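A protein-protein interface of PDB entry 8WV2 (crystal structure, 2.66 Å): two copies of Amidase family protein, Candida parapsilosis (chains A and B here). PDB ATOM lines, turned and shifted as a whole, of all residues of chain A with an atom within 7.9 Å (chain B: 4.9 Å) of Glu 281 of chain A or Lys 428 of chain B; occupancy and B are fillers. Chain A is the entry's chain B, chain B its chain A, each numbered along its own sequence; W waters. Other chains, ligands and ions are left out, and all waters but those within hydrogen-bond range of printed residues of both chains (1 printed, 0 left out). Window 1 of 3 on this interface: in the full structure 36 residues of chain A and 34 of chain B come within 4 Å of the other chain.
Leu 265 of chain A touches none of the printed residues of chain B. Printed residues of chain B within 4 Å of Arg 278 of chain A: Leu 426 (3.9 Å). Glu 281 of chain A touches just these residues of chain B: Asn 425 (3.5 Å), Lys 428 (2.9 Å) and Gln 429 (3.0 Å). Of the printed residues of chain B, Thr 315 of chain A touches Gln 429 (3.5 Å). Printed residues of chain A within 4 Å of Asn 425 of chain B: Gly 279 (3.0 Å) and Glu 281 (3.5 Å). Printed residues of chain A within 4 Å of Leu 426 of chain B: Arg 278 and Gly 279. Lys 428 of chain B touches just one residue of chain A: Glu 281 (2.9 Å). Printed residues of chain A within 4 Å of Arg 432 of chain B: Pro 314. The nearest residue of chain A that does not touch Lys 428 of chain B is Gly 279 of chain A (6.6 Å).
7 positions are printed for both chains.
The backbone carbonyl oxygen (O) of Gly 279 of chain A is in hydrogen-bond range of the side-chain amide nitrogen (ND2) of Asn 425 of chain B. OE2 of Glu 281 of chain A is in salt-bridge range of NZ of Lys 428 of chain B, at 2.9 Å. NE2 of Gln 429 of chain B is in hydrogen-bond range of OE1 of Glu 281 of chain A (3.0 Å).
Among the printed residues, merely in contact across the chains: Arg 278 of chain A with Leu 426 of chain B, Gly 279 of chain A with Leu 426 of chain B, Glu 281 of chain A with Asn 425 of chain B, Pro 314 of chain A with Arg 432 of chain B and Thr 315 of chain A with Gln 429 of chain B.
Of the 14 printed residues of chain B, 5 touch a printed residue of chain A. Hydrophobic or aromatic side chains of chain B that line the printed part of chain A: Leu 426. Hydrophobic or aromatic side chains of chain A within 4 Å of the printed part of chain B: Pro 314. Along chain A the printed residues that touch a printed residue of chain B span positions 278 to 315. Among the printed residues, 8 pairs touch across the chains.
O of Ser 282 of chain B sits at hydrogen-bond distance from NZ of Lys 428 of chain B (3.0 Å). NZ of Lys 428 of chain B is in hydrogen-bond range of OD1 of Asn 425 of chain B (2.9 Å). The side-chain amide oxygen (OE1) of Gln 429 of chain B lies within hydrogen-bond range of the guanidinium group (NH1) of Arg 432 of chain B (3.4 Å). The backbone carbonyl oxygen (O) of Leu 479 of chain B is in hydrogen-bond range of the guanidinium group (NE) of Arg 432 of chain B (2.8 Å).
Water W1 lies within hydrogen-bond range of the side-chain carboxylate of Glu 281 of chain A and the backbone NH of Ser 282 of chain B.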
ATOM      1  N   LEU A 265       3.071   2.726  24.763  1.00  0.00           N
ATOM      2  CA  LEU A 265       1.958   2.458  25.663  1.00  0.00           C
ATOM      3  C   LEU A 265       1.923   0.972  25.982  1.00  0.00           C
ATOM      4  O   LEU A 265       2.050   0.135  25.087  1.00  0.00           O
ATOM      5  CB  LEU A 265       0.638   2.888  25.026  1.00  0.00           C
ATOM      6  CG  LEU A 265      -0.626   2.572  25.833  1.00  0.00           C
ATOM      7  CD1 LEU A 265      -0.648   3.370  27.136  1.00  0.00           C
ATOM      8  CD2 LEU A 265      -1.873   2.835  25.025  1.00  0.00           C
ATOM      9  N   ASN A 277     -10.698  14.337  31.603  1.00  0.00           N
ATOM     10  CA  ASN A 277     -11.257  13.288  30.746  1.00  0.00           C
ATOM     11  C   ASN A 277     -10.905  11.889  31.240  1.00  0.00           C
ATOM     12  O   ASN A 277     -10.475  11.024  30.474  1.00  0.00           O
ATOM     13  CB  ASN A 277     -10.824  13.473  29.297  1.00  0.00           C
ATOM     14  CG  ASN A 277     -10.882  14.901  28.869  1.00  0.00           C
ATOM     15  OD1 ASN A 277      -9.992  15.387  28.184  1.00  0.00           O
ATOM     16  ND2 ASN A 277     -11.915  15.605  29.305  1.00  0.00           N
ATOM     17  N   ARG A 278     -11.074  11.681  32.538  1.00  0.00           N
ATOM     18  CA  ARG A 278     -10.827  10.368  33.110  1.00  0.00           C
ATOM     19  C   ARG A 278     -11.858   9.368  32.595  1.00  0.00           C
ATOM     20  O   ARG A 278     -13.068   9.629  32.615  1.00  0.00           O
ATOM     21  CB  ARG A 278     -10.859  10.452  34.631  1.00  0.00           C
ATOM     22  CG  ARG A 278      -9.680  11.194  35.218  1.00  0.00           C
ATOM     23  CD  ARG A 278      -9.677  11.082  36.724  1.00  0.00           C
ATOM     24  NE  ARG A 278     -10.794  11.825  37.304  1.00  0.00           N
ATOM     25  CZ  ARG A 278     -11.193  11.725  38.570  1.00  0.00           C
ATOM     26  NH1 ARG A 278     -10.591  10.869  39.387  1.00  0.00           N
ATOM     27  NH2 ARG A 278     -12.217  12.452  39.011  1.00  0.00           N
ATOM     28  N   GLY A 279     -11.371   8.221  32.121  1.00  0.00           N
ATOM     29  CA  GLY A 279     -12.178   7.230  31.449  1.00  0.00           C
ATOM     30  C   GLY A 279     -12.141   7.319  29.937  1.00  0.00           C
ATOM     31  O   GLY A 279     -12.504   6.351  29.264  1.00  0.00           O
ATOM     32  N   SER A 280     -11.675   8.438  29.389  1.00  0.00           N
ATOM     33  CA  SER A 280     -11.484   8.538  27.952  1.00  0.00           C
ATOM     34  C   SER A 280     -10.321   7.660  27.515  1.00  0.00           C
ATOM     35  O   SER A 280      -9.212   7.754  28.061  1.00  0.00           O
ATOM     36  CB  SER A 280     -11.233   9.984  27.541  1.00  0.00           C
ATOM     37  OG  SER A 280     -11.210  10.092  26.129  1.00  0.00           O
ATOM     38  N   GLU A 281     -10.581   6.803  26.531  1.00  0.00           N
ATOM     39  CA  GLU A 281      -9.587   5.859  26.060  1.00  0.00           C
ATOM     40  C   GLU A 281      -9.264   5.996  24.580  1.00  0.00           C
ATOM     41  O   GLU A 281      -8.408   5.257  24.083  1.00  0.00           O
ATOM     42  CB  GLU A 281     -10.042   4.431  26.377  1.00  0.00           C
ATOM     43  CG  GLU A 281     -10.017   4.138  27.860  1.00  0.00           C
ATOM     44  CD  GLU A 281     -10.403   2.719  28.188  1.00  0.00           C
ATOM     45  OE1 GLU A 281     -10.466   2.392  29.390  1.00  0.00           O
ATOM     46  OE2 GLU A 281     -10.628   1.927  27.252  1.00  0.00           O
ATOM     47  N   SER A 282      -9.926   6.900  23.854  1.00  0.00           N
ATOM     48  CA  SER A 282      -9.704   6.988  22.414  1.00  0.00           C
ATOM     49  C   SER A 282      -8.245   7.301  22.082  1.00  0.00           C
ATOM     50  O   SER A 282      -7.677   6.730  21.142  1.00  0.00           O
ATOM     51  CB  SER A 282     -10.641   8.031  21.810  1.00  0.00           C
ATOM     52  OG  SER A 282     -11.986   7.664  22.063  1.00  0.00           O
ATOM     53  N   ILE A 283      -7.628   8.215  22.827  1.00  0.00           N
ATOM     54  CA  ILE A 283      -6.196   8.479  22.752  1.00  0.00           C
ATOM     55  C   ILE A 283      -5.656   8.475  24.176  1.00  0.00           C
ATOM     56  O   ILE A 283      -6.112   9.268  25.010  1.00  0.00           O
ATOM     57  CB  ILE A 283      -5.891   9.820  22.066  1.00  0.00           C
ATOM     58  CG1 ILE A 283      -6.397   9.820  20.627  1.00  0.00           C
ATOM     59  CG2 ILE A 283      -4.401  10.095  22.098  1.00  0.00           C
ATOM     60  CD1 ILE A 283      -5.584   8.944  19.701  1.00  0.00           C
ATOM     61  N   LEU A 284      -4.659   7.629  24.443  1.00  0.00           N
ATOM     62  CA  LEU A 284      -4.144   7.420  25.794  1.00  0.00           C
ATOM     63  C   LEU A 284      -2.782   8.088  25.997  1.00  0.00           C
ATOM     64  O   LEU A 284      -1.933   8.104  25.099  1.00  0.00           O
ATOM     65  CB  LEU A 284      -4.043   5.922  26.123  1.00  0.00           C
ATOM     66  CG  LEU A 284      -5.348   5.163  26.390  1.00  0.00           C
ATOM     67  CD1 LEU A 284      -5.167   3.627  26.362  1.00  0.00           C
ATOM     68  CD2 LEU A 284      -5.922   5.627  27.730  1.00  0.00           C
ATOM     69  N   SER A 285      -2.603   8.677  27.178  1.00  0.00           N
ATOM     70  CA  SER A 285      -1.319   9.221  27.590  1.00  0.00           C
ATOM     71  C   SER A 285      -0.363   8.099  27.994  1.00  0.00           C
ATOM     72  O   SER A 285      -0.775   6.994  28.347  1.00  0.00           O
ATOM     73  CB  SER A 285      -1.513  10.200  28.747  1.00  0.00           C
ATOM     74  OG  SER A 285      -0.281  10.670  29.248  1.00  0.00           O
ATOM     75  N   PRO A 314      -2.665  -4.640  34.667  1.00  0.00           N
ATOM     76  CA  PRO A 314      -2.919  -5.636  33.617  1.00  0.00           C
ATOM     77  C   PRO A 314      -3.010  -5.067  32.207  1.00  0.00           C
ATOM     78  O   PRO A 314      -3.208  -5.846  31.263  1.00  0.00           O
ATOM     79  CB  PRO A 314      -4.262  -6.249  34.046  1.00  0.00           C
ATOM     80  CG  PRO A 314      -4.955  -5.156  34.784  1.00  0.00           C
ATOM     81  CD  PRO A 314      -3.879  -4.308  35.435  1.00  0.00           C
ATOM     82  N   THR A 315      -2.869  -3.750  32.029  1.00  0.00           N
ATOM     83  CA  THR A 315      -2.820  -3.165  30.694  1.00  0.00           C
ATOM     84  C   THR A 315      -1.455  -3.288  30.043  1.00  0.00           C
ATOM     85  O   THR A 315      -1.303  -2.881  28.889  1.00  0.00           O
ATOM     86  CB  THR A 315      -3.228  -1.687  30.722  1.00  0.00           C
ATOM     87  OG1 THR A 315      -2.413  -0.986  31.668  1.00  0.00           O
ATOM     88  CG2 THR A 315      -4.719  -1.532  31.060  1.00  0.00           C
ATOM     89  N   LEU A 383     -10.724  13.688  19.074  1.00  0.00           N
ATOM     90  CA  LEU A 383     -10.578  12.692  20.124  1.00  0.00           C
ATOM     91  C   LEU A 383      -9.892  13.206  21.388  1.00  0.00           C
ATOM     92  O   LEU A 383     -10.078  12.602  22.450  1.00  0.00           O
ATOM     93  CB  LEU A 383      -9.828  11.467  19.586  1.00  0.00           C
ATOM     94  CG  LEU A 383     -10.589  10.647  18.534  1.00  0.00           C
ATOM     95  CD1 LEU A 383      -9.783   9.437  18.067  1.00  0.00           C
ATOM     96  CD2 LEU A 383     -11.942  10.226  19.085  1.00  0.00           C
ATOM     97  N   GLU A 386     -13.220  14.620  23.542  1.00  0.00           N
ATOM     98  CA  GLU A 386     -14.339  13.989  22.853  1.00  0.00           C
ATOM     99  C   GLU A 386     -15.678  14.271  23.515  1.00  0.00           C
ATOM    100  O   GLU A 386     -16.718  13.942  22.933  1.00  0.00           O
ATOM    101  CB  GLU A 386     -14.126  12.471  22.726  1.00  0.00           C
ATOM    102  CG  GLU A 386     -13.681  11.738  23.988  1.00  0.00           C
ATOM    103  CD  GLU A 386     -13.504  10.242  23.748  1.00  0.00           C
ATOM    104  OE1 GLU A 386     -13.508   9.839  22.567  1.00  0.00           O
ATOM    105  OE2 GLU A 386     -13.372   9.472  24.726  1.00  0.00           O
ATOM    106  N   GLN A 421     -17.706   8.801  17.826  1.00  0.00           N
ATOM    107  CA  GLN A 421     -16.477   8.204  18.330  1.00  0.00           C
ATOM    108  C   GLN A 421     -16.102   6.974  17.506  1.00  0.00           C
ATOM    109  O   GLN A 421     -14.931   6.769  17.170  1.00  0.00           O
ATOM    110  CB  GLN A 421     -16.619   7.860  19.817  1.00  0.00           C
ATOM    111  CG  GLN A 421     -15.343   7.290  20.425  1.00  0.00           C
ATOM    112  CD  GLN A 421     -15.525   6.753  21.825  1.00  0.00           C
ATOM    113  OE1 GLN A 421     -16.086   5.681  22.020  1.00  0.00           O
ATOM    114  NE2 GLN A 421     -15.007   7.474  22.807  1.00  0.00           N
ATOM    115  N   ASN A 425     -12.588   6.657  15.766  1.00  0.00           N
ATOM    116  CA  ASN A 425     -11.736   5.528  16.119  1.00  0.00           C
ATOM    117  C   ASN A 425     -11.303   4.766  14.868  1.00  0.00           C
ATOM    118  O   ASN A 425     -10.140   4.363  14.747  1.00  0.00           O
ATOM    119  CB  ASN A 425     -12.468   4.595  17.089  1.00  0.00           C
ATOM    120  CG  ASN A 425     -12.372   5.048  18.545  1.00  0.00           C
ATOM    121  OD1 ASN A 425     -11.520   5.868  18.901  1.00  0.00           O
ATOM    122  ND2 ASN A 425     -13.252   4.516  19.390  1.00  0.00           N
ATOM    123  N   LYS A 428      -8.707   6.695  13.182  1.00  0.00           N
ATOM    124  CA  LYS A 428      -7.463   6.555  13.931  1.00  0.00           C
ATOM    125  C   LYS A 428      -6.775   5.237  13.595  1.00  0.00           C
ATOM    126  O   LYS A 428      -5.579   5.208  13.288  1.00  0.00           O
ATOM    127  CB  LYS A 428      -7.752   6.670  15.430  1.00  0.00           C
ATOM    128  CG  LYS A 428      -6.642   6.194  16.339  1.00  0.00           C
ATOM    129  CD  LYS A 428      -7.133   6.124  17.777  1.00  0.00           C
ATOM    130  CE  LYS A 428      -8.170   5.014  17.929  1.00  0.00           C
ATOM    131  NZ  LYS A 428      -8.860   5.009  19.254  1.00  0.00           N
ATOM    132  N   GLN A 429      -7.527   4.133  13.624  1.00  0.00           N
ATOM    133  CA  GLN A 429      -6.917   2.837  13.352  1.00  0.00           C
ATOM    134  C   GLN A 429      -6.492   2.720  11.893  1.00  0.00           C
ATOM    135  O   GLN A 429      -5.445   2.129  11.593  1.00  0.00           O
ATOM    136  CB  GLN A 429      -7.881   1.715  13.734  1.00  0.00           C
ATOM    137  CG  GLN A 429      -8.291   1.713  15.210  1.00  0.00           C
ATOM    138  CD  GLN A 429      -7.144   1.419  16.183  1.00  0.00           C
ATOM    139  OE1 GLN A 429      -5.997   1.208  15.786  1.00  0.00           O
ATOM    140  NE2 GLN A 429      -7.471   1.375  17.470  1.00  0.00           N
ATOM    141  N   ARG A 432      -3.241   4.771  11.566  1.00  0.00           N
ATOM    142  CA  ARG A 432      -2.146   3.994  12.144  1.00  0.00           C
ATOM    143  C   ARG A 432      -1.714   2.876  11.205  1.00  0.00           C
ATOM    144  O   ARG A 432      -0.517   2.662  10.991  1.00  0.00           O
ATOM    145  CB  ARG A 432      -2.565   3.409  13.494  1.00  0.00           C
ATOM    146  CG  ARG A 432      -2.770   4.436  14.603  1.00  0.00           C
ATOM    147  CD  ARG A 432      -3.385   3.798  15.850  1.00  0.00           C
ATOM    148  NE  ARG A 432      -3.341   4.683  17.016  1.00  0.00           N
ATOM    149  CZ  ARG A 432      -3.880   4.386  18.195  1.00  0.00           C
ATOM    150  NH1 ARG A 432      -4.504   3.228  18.365  1.00  0.00           N
ATOM    151  NH2 ARG A 432      -3.799   5.246  19.204  1.00  0.00           N
ATOM    152  N   SER B 282     -14.477  -0.082  23.481  1.00  0.00           N
ATOM    153  CA  SER B 282     -14.575  -0.285  24.927  1.00  0.00           C
ATOM    154  C   SER B 282     -14.338  -1.741  25.315  1.00  0.00           C
ATOM    155  O   SER B 282     -13.647  -2.023  26.302  1.00  0.00           O
ATOM    156  CB  SER B 282     -15.951   0.161  25.425  1.00  0.00           C
ATOM    157  OG  SER B 282     -16.198   1.529  25.149  1.00  0.00           O
ATOM    158  N   ILE B 283     -14.915  -2.678  24.565  1.00  0.00           N
ATOM    159  CA  ILE B 283     -14.655  -4.106  24.720  1.00  0.00           C
ATOM    160  C   ILE B 283     -14.341  -4.638  23.331  1.00  0.00           C
ATOM    161  O   ILE B 283     -15.140  -4.457  22.407  1.00  0.00           O
ATOM    162  CB  ILE B 283     -15.857  -4.851  25.329  1.00  0.00           C
ATOM    163  CG1 ILE B 283     -16.183  -4.291  26.716  1.00  0.00           C
ATOM    164  CG2 ILE B 283     -15.576  -6.338  25.416  1.00  0.00           C
ATOM    165  CD1 ILE B 283     -15.150  -4.625  27.771  1.00  0.00           C
ATOM    166  N   ILE B 379     -20.915  -4.462  33.926  1.00  0.00           N
ATOM    167  CA  ILE B 379     -20.051  -3.653  33.069  1.00  0.00           C
ATOM    168  C   ILE B 379     -20.317  -3.965  31.604  1.00  0.00           C
ATOM    169  O   ILE B 379     -20.552  -3.061  30.791  1.00  0.00           O
ATOM    170  CB  ILE B 379     -18.568  -3.874  33.420  1.00  0.00           C
ATOM    171  CG1 ILE B 379     -18.267  -3.434  34.849  1.00  0.00           C
ATOM    172  CG2 ILE B 379     -17.686  -3.092  32.471  1.00  0.00           C
ATOM    173  CD1 ILE B 379     -16.890  -3.851  35.320  1.00  0.00           C
ATOM    174  N   LEU B 383     -21.258  -1.874  27.964  1.00  0.00           N
ATOM    175  CA  LEU B 383     -20.223  -1.653  26.962  1.00  0.00           C
ATOM    176  C   LEU B 383     -20.372  -2.516  25.708  1.00  0.00           C
ATOM    177  O   LEU B 383     -19.813  -2.155  24.667  1.00  0.00           O
ATOM    178  CB  LEU B 383     -18.844  -1.886  27.591  1.00  0.00           C
ATOM    179  CG  LEU B 383     -18.467  -0.884  28.695  1.00  0.00           C
ATOM    180  CD1 LEU B 383     -17.105  -1.197  29.284  1.00  0.00           C
ATOM    181  CD2 LEU B 383     -18.515   0.554  28.198  1.00  0.00           C
ATOM    182  N   TRP B 424     -17.853   3.829  32.887  1.00  0.00           N
ATOM    183  CA  TRP B 424     -17.794   2.379  32.778  1.00  0.00           C
ATOM    184  C   TRP B 424     -16.446   1.877  32.273  1.00  0.00           C
ATOM    185  O   TRP B 424     -16.064   0.743  32.586  1.00  0.00           O
ATOM    186  CB  TRP B 424     -18.937   1.904  31.898  1.00  0.00           C
ATOM    187  CG  TRP B 424     -20.238   2.052  32.603  1.00  0.00           C
ATOM    188  CD1 TRP B 424     -21.223   2.957  32.340  1.00  0.00           C
ATOM    189  CD2 TRP B 424     -20.678   1.296  33.734  1.00  0.00           C
ATOM    190  NE1 TRP B 424     -22.262   2.793  33.223  1.00  0.00           N
ATOM    191  CE2 TRP B 424     -21.951   1.780  34.092  1.00  0.00           C
ATOM    192  CE3 TRP B 424     -20.123   0.246  34.473  1.00  0.00           C
ATOM    193  CZ2 TRP B 424     -22.681   1.249  35.152  1.00  0.00           C
ATOM    194  CZ3 TRP B 424     -20.850  -0.279  35.529  1.00  0.00           C
ATOM    195  CH2 TRP B 424     -22.115   0.223  35.857  1.00  0.00           C
ATOM    196  N   ASN B 425     -15.715   2.687  31.500  1.00  0.00           N
ATOM    197  CA  ASN B 425     -14.322   2.357  31.218  1.00  0.00           C
ATOM    198  C   ASN B 425     -13.501   2.316  32.501  1.00  0.00           C
ATOM    199  O   ASN B 425     -12.696   1.397  32.700  1.00  0.00           O
ATOM    200  CB  ASN B 425     -13.725   3.359  30.229  1.00  0.00           C
ATOM    201  CG  ASN B 425     -14.068   3.031  28.791  1.00  0.00           C
ATOM    202  OD1 ASN B 425     -14.504   1.920  28.481  1.00  0.00           O
ATOM    203  ND2 ASN B 425     -13.858   3.990  27.900  1.00  0.00           N
ATOM    204  N   LEU B 426     -13.716   3.290  33.397  1.00  0.00           N
ATOM    205  CA  LEU B 426     -13.056   3.275  34.700  1.00  0.00           C
ATOM    206  C   LEU B 426     -13.476   2.067  35.525  1.00  0.00           C
ATOM    207  O   LEU B 426     -12.640   1.452  36.201  1.00  0.00           O
ATOM    208  CB  LEU B 426     -13.363   4.564  35.466  1.00  0.00           C
ATOM    209  CG  LEU B 426     -12.755   5.839  34.889  1.00  0.00           C
ATOM    210  CD1 LEU B 426     -13.318   7.076  35.566  1.00  0.00           C
ATOM    211  CD2 LEU B 426     -11.233   5.769  35.053  1.00  0.00           C
ATOM    212  N   GLN B 427     -14.769   1.719  35.495  1.00  0.00           N
ATOM    213  CA  GLN B 427     -15.217   0.501  36.162  1.00  0.00           C
ATOM    214  C   GLN B 427     -14.530  -0.718  35.568  1.00  0.00           C
ATOM    215  O   GLN B 427     -14.139  -1.643  36.293  1.00  0.00           O
ATOM    216  CB  GLN B 427     -16.732   0.370  36.038  1.00  0.00           C
ATOM    217  CG  GLN B 427     -17.517   1.389  36.826  1.00  0.00           C
ATOM    218  CD  GLN B 427     -17.453   1.147  38.306  1.00  0.00           C
ATOM    219  OE1 GLN B 427     -17.391   2.091  39.093  1.00  0.00           O
ATOM    220  NE2 GLN B 427     -17.478  -0.121  38.704  1.00  0.00           N
ATOM    221  N   LYS B 428     -14.369  -0.726  34.245  1.00  0.00           N
ATOM    222  CA  LYS B 428     -13.725  -1.843  33.565  1.00  0.00           C
ATOM    223  C   LYS B 428     -12.264  -1.953  33.978  1.00  0.00           C
ATOM    224  O   LYS B 428     -11.793  -3.032  34.354  1.00  0.00           O
ATOM    225  CB  LYS B 428     -13.863  -1.664  32.052  1.00  0.00           C
ATOM    226  CG  LYS B 428     -12.967  -2.544  31.214  1.00  0.00           C
ATOM    227  CD  LYS B 428     -12.982  -2.088  29.765  1.00  0.00           C
ATOM    228  CE  LYS B 428     -12.265  -0.745  29.621  1.00  0.00           C
ATOM    229  NZ  LYS B 428     -12.429  -0.138  28.269  1.00  0.00           N
ATOM    230  N   GLN B 429     -11.534  -0.841  33.935  1.00  0.00           N
ATOM    231  CA  GLN B 429     -10.118  -0.896  34.281  1.00  0.00           C
ATOM    232  C   GLN B 429      -9.932  -1.186  35.766  1.00  0.00           C
ATOM    233  O   GLN B 429      -8.988  -1.883  36.156  1.00  0.00           O
ATOM    234  CB  GLN B 429      -9.425   0.411  33.893  1.00  0.00           C
ATOM    235  CG  GLN B 429      -9.495   0.774  32.419  1.00  0.00           C
ATOM    236  CD  GLN B 429      -8.739  -0.189  31.498  1.00  0.00           C
ATOM    237  OE1 GLN B 429      -8.111  -1.151  31.944  1.00  0.00           O
ATOM    238  NE2 GLN B 429      -8.807   0.075  30.200  1.00  0.00           N
ATOM    239  N   ALA B 430     -10.826  -0.669  36.609  1.00  0.00           N
ATOM    240  CA  ALA B 430     -10.737  -0.967  38.035  1.00  0.00           C
ATOM    241  C   ALA B 430     -10.931  -2.458  38.297  1.00  0.00           C
ATOM    242  O   ALA B 430     -10.146  -3.080  39.024  1.00  0.00           O
ATOM    243  CB  ALA B 430     -11.760  -0.139  38.810  1.00  0.00           C
ATOM    244  N   TYR B 431     -11.965  -3.051  37.693  1.00  0.00           N
ATOM    245  CA  TYR B 431     -12.209  -4.480  37.854  1.00  0.00           C
ATOM    246  C   TYR B 431     -11.021  -5.308  37.376  1.00  0.00           C
ATOM    247  O   TYR B 431     -10.618  -6.271  38.037  1.00  0.00           O
ATOM    248  CB  TYR B 431     -13.483  -4.878  37.110  1.00  0.00           C
ATOM    249  CG  TYR B 431     -13.832  -6.337  37.267  1.00  0.00           C
ATOM    250  CD1 TYR B 431     -14.478  -6.790  38.408  1.00  0.00           C
ATOM    251  CD2 TYR B 431     -13.524  -7.261  36.274  1.00  0.00           C
ATOM    252  CE1 TYR B 431     -14.805  -8.120  38.564  1.00  0.00           C
ATOM    253  CE2 TYR B 431     -13.847  -8.597  36.422  1.00  0.00           C
ATOM    254  CZ  TYR B 431     -14.491  -9.019  37.570  1.00  0.00           C
ATOM    255  OH  TYR B 431     -14.812 -10.345  37.730  1.00  0.00           O
ATOM    256  N   ARG B 432     -10.455  -4.955  36.218  1.00  0.00           N
ATOM    257  CA  ARG B 432      -9.287  -5.668  35.716  1.00  0.00           C
ATOM    258  C   ARG B 432      -8.144  -5.626  36.721  1.00  0.00           C
ATOM    259  O   ARG B 432      -7.482  -6.644  36.967  1.00  0.00           O
ATOM    260  CB  ARG B 432      -8.845  -5.070  34.382  1.00  0.00           C
ATOM    261  CG  ARG B 432      -9.828  -5.298  33.239  1.00  0.00           C
ATOM    262  CD  ARG B 432      -9.421  -4.509  32.018  1.00  0.00           C
ATOM    263  NE  ARG B 432     -10.188  -4.901  30.843  1.00  0.00           N
ATOM    264  CZ  ARG B 432     -10.090  -4.302  29.659  1.00  0.00           C
ATOM    265  NH1 ARG B 432      -9.254  -3.279  29.496  1.00  0.00           N
ATOM    266  NH2 ARG B 432     -10.830  -4.723  28.641  1.00  0.00           N
ATOM    267  N   LEU B 479     -14.099  -9.560  29.496  1.00  0.00           N
ATOM    268  CA  LEU B 479     -13.927  -8.344  30.282  1.00  0.00           C
ATOM    269  C   LEU B 479     -12.477  -8.184  30.737  1.00  0.00           C
ATOM    270  O   LEU B 479     -11.942  -7.068  30.764  1.00  0.00           O
ATOM    271  CB  LEU B 479     -14.882  -8.360  31.477  1.00  0.00           C
ATOM    272  CG  LEU B 479     -14.856  -7.140  32.409  1.00  0.00           C
ATOM    273  CD1 LEU B 479     -15.022  -5.858  31.606  1.00  0.00           C
ATOM    274  CD2 LEU B 479     -15.946  -7.240  33.479  1.00  0.00           C
HETATM  275  O   HOH W   1     -11.765   1.565  24.950  1.00  0.00           O
